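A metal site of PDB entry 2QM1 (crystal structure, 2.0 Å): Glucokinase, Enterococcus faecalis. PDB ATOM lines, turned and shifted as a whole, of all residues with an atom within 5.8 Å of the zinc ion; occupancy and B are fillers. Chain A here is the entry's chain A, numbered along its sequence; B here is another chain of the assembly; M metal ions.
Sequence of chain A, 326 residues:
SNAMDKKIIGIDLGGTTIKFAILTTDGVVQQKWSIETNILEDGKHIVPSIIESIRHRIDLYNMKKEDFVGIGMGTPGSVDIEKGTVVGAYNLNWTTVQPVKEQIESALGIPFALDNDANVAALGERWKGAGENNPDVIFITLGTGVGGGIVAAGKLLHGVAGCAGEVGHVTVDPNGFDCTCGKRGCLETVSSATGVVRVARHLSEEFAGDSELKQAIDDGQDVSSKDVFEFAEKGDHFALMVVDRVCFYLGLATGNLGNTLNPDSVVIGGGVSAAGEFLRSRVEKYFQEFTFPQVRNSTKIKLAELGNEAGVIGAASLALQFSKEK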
ATOM      1  N   GLY A 168      31.905   5.951 -10.860  1.00  0.00           N
ATOM      2  CA  GLY A 168      31.059   5.389 -11.887  1.00  0.00           C
ATOM      3  C   GLY A 168      29.785   6.195 -12.017  1.00  0.00           C
ATOM      4  O   GLY A 168      29.041   6.021 -12.965  1.00  0.00           O
ATOM      5  N   HIS A 169      29.526   7.068 -11.039  1.00  0.00           N
ATOM      6  CA  HIS A 169      28.321   7.913 -11.076  1.00  0.00           C
ATOM      7  C   HIS A 169      28.581   9.366 -11.200  1.00  0.00           C
ATOM      8  O   HIS A 169      27.819  10.203 -10.744  1.00  0.00           O
ATOM      9  CB  HIS A 169      27.399   7.605  -9.924  1.00  0.00           C
ATOM     10  CG  HIS A 169      26.887   6.216  -9.994  1.00  0.00           C
ATOM     11  ND1 HIS A 169      25.797   5.863 -10.772  1.00  0.00           N
ATOM     12  CD2 HIS A 169      27.381   5.068  -9.493  1.00  0.00           C
ATOM     13  CE1 HIS A 169      25.631   4.563 -10.705  1.00  0.00           C
ATOM     14  NE2 HIS A 169      26.584   4.050  -9.937  1.00  0.00           N
ATOM     15  N   CYS A 179      20.782   5.813 -15.758  1.00  0.00           N
ATOM     16  CA  CYS A 179      21.566   4.993 -14.880  1.00  0.00           C
ATOM     17  C   CYS A 179      20.702   4.374 -13.813  1.00  0.00           C
ATOM     18  O   CYS A 179      19.669   4.936 -13.427  1.00  0.00           O
ATOM     19  CB  CYS A 179      22.688   5.796 -14.236  1.00  0.00           C
ATOM     20  SG  CYS A 179      23.815   4.790 -13.346  1.00  0.00           S
ATOM     21  N   THR A 180      21.120   3.215 -13.338  1.00  0.00           N
ATOM     22  CA  THR A 180      20.507   2.563 -12.190  1.00  0.00           C
ATOM     23  C   THR A 180      20.285   3.467 -10.975  1.00  0.00           C
ATOM     24  O   THR A 180      19.427   3.217 -10.154  1.00  0.00           O
ATOM     25  CB  THR A 180      21.358   1.356 -11.704  1.00  0.00           C
ATOM     26  OG1 THR A 180      21.014   1.066 -10.362  1.00  0.00           O
ATOM     27  CG2 THR A 180      22.829   1.629 -11.714  1.00  0.00           C
ATOM     28  N   CYS A 181      21.125   4.500 -10.837  1.00  0.00           N
ATOM     29  CA  CYS A 181      21.103   5.342  -9.661  1.00  0.00           C
ATOM     30  C   CYS A 181      19.961   6.349  -9.698  1.00  0.00           C
ATOM     31  O   CYS A 181      19.581   6.848  -8.643  1.00  0.00           O
ATOM     32  CB  CYS A 181      22.469   6.035  -9.439  1.00  0.00           C
ATOM     33  SG  CYS A 181      22.807   7.468 -10.462  1.00  0.00           S
ATOM     34  N   GLY A 182      19.409   6.633 -10.884  1.00  0.00           N
ATOM     35  CA  GLY A 182      18.249   7.531 -11.016  1.00  0.00           C
ATOM     36  C   GLY A 182      18.521   8.724 -11.912  1.00  0.00           C
ATOM     37  O   GLY A 182      17.607   9.434 -12.299  1.00  0.00           O
ATOM     38  N   LYS A 183      19.782   8.929 -12.277  1.00  0.00           N
ATOM     39  CA  LYS A 183      20.071  10.067 -13.141  1.00  0.00           C
ATOM     40  C   LYS A 183      20.654   9.633 -14.489  1.00  0.00           C
ATOM     41  O   LYS A 183      20.853   8.465 -14.719  1.00  0.00           O
ATOM     42  CB  LYS A 183      20.956  11.062 -12.413  1.00  0.00           C
ATOM     43  CG  LYS A 183      22.330  10.549 -12.136  1.00  0.00           C
ATOM     44  CD  LYS A 183      23.104  11.579 -11.283  1.00  0.00           C
ATOM     45  CE  LYS A 183      24.441  11.009 -10.775  1.00  0.00           C
ATOM     46  NZ  LYS A 183      25.483  11.116 -11.821  1.00  0.00           N
ATOM     47  N   CYS A 186      25.643   8.642 -16.427  1.00  0.00           N
ATOM     48  CA  CYS A 186      26.730   8.239 -15.522  1.00  0.00           C
ATOM     49  C   CYS A 186      27.784   7.455 -16.283  1.00  0.00           C
ATOM     50  O   CYS A 186      27.438   6.729 -17.206  1.00  0.00           O
ATOM     51  CB  CYS A 186      26.216   7.403 -14.364  1.00  0.00           C
ATOM     52  SG  CYS A 186      25.170   8.338 -13.246  1.00  0.00           S
ATOM     53  N   GLU A 188      29.344   4.782 -15.573  1.00  0.00           N
ATOM     54  CA  GLU A 188      29.019   3.360 -15.510  1.00  0.00           C
ATOM     55  C   GLU A 188      28.160   2.936 -16.686  1.00  0.00           C
ATOM     56  O   GLU A 188      28.133   1.789 -17.102  1.00  0.00           O
ATOM     57  CB  GLU A 188      28.262   3.003 -14.216  1.00  0.00           C
ATOM     58  CG  GLU A 188      28.181   1.472 -13.976  1.00  0.00           C
ATOM     59  CD  GLU A 188      27.900   1.091 -12.528  1.00  0.00           C
ATOM     60  OE1 GLU A 188      28.856   0.954 -11.723  1.00  0.00           O
ATOM     61  OE2 GLU A 188      26.713   0.935 -12.188  1.00  0.00           O
ATOM     62  N   PHE B 292      24.118  11.417  -7.273  1.00  0.00           N
ATOM     63  CA  PHE B 292      23.445  10.189  -6.896  1.00  0.00           C
ATOM     64  C   PHE B 292      22.794  10.298  -5.503  1.00  0.00           C
ATOM     65  O   PHE B 292      23.146  11.165  -4.744  1.00  0.00           O
ATOM     66  CB  PHE B 292      24.284   8.914  -7.176  1.00  0.00           C
ATOM     67  CG  PHE B 292      25.520   8.771  -6.334  1.00  0.00           C
ATOM     68  CD1 PHE B 292      26.752   9.176  -6.810  1.00  0.00           C
ATOM     69  CD2 PHE B 292      25.461   8.149  -5.111  1.00  0.00           C
ATOM     70  CE1 PHE B 292      27.914   9.018  -6.045  1.00  0.00           C
ATOM     71  CE2 PHE B 292      26.594   7.988  -4.331  1.00  0.00           C
ATOM     72  CZ  PHE B 292      27.814   8.433  -4.783  1.00  0.00           C
HETATM   73 ZN    ZN M   1      24.519   6.621 -11.854  1.00  0.00          ZN
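The side-chain amino group of Lys 183 sits at hydrogen-bond distance from the backbone carbonyl oxygen of His 169 (2.7 Å).
The side-chain sulfur (SG) of Cys 186 lies close to the side-chain amino group (NZ) of Lys 183, at 3.1 Å.
Within 4 Å of the zinc ion: His 169, Cys 179, Cys 181 and Cys 186.
The nearest printed residue that does not touch the zinc ion is Lys 183 (4.5 Å).
ND1 of His 169 binds the zinc ion.
The zinc ion is bound by SG of Cys 186 (2.3 Å).
SG of Cys 181 binds the zinc ion, at 2.4 Å.
SG of Cys 179 is bound to the zinc ion, at 2.5 Å.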
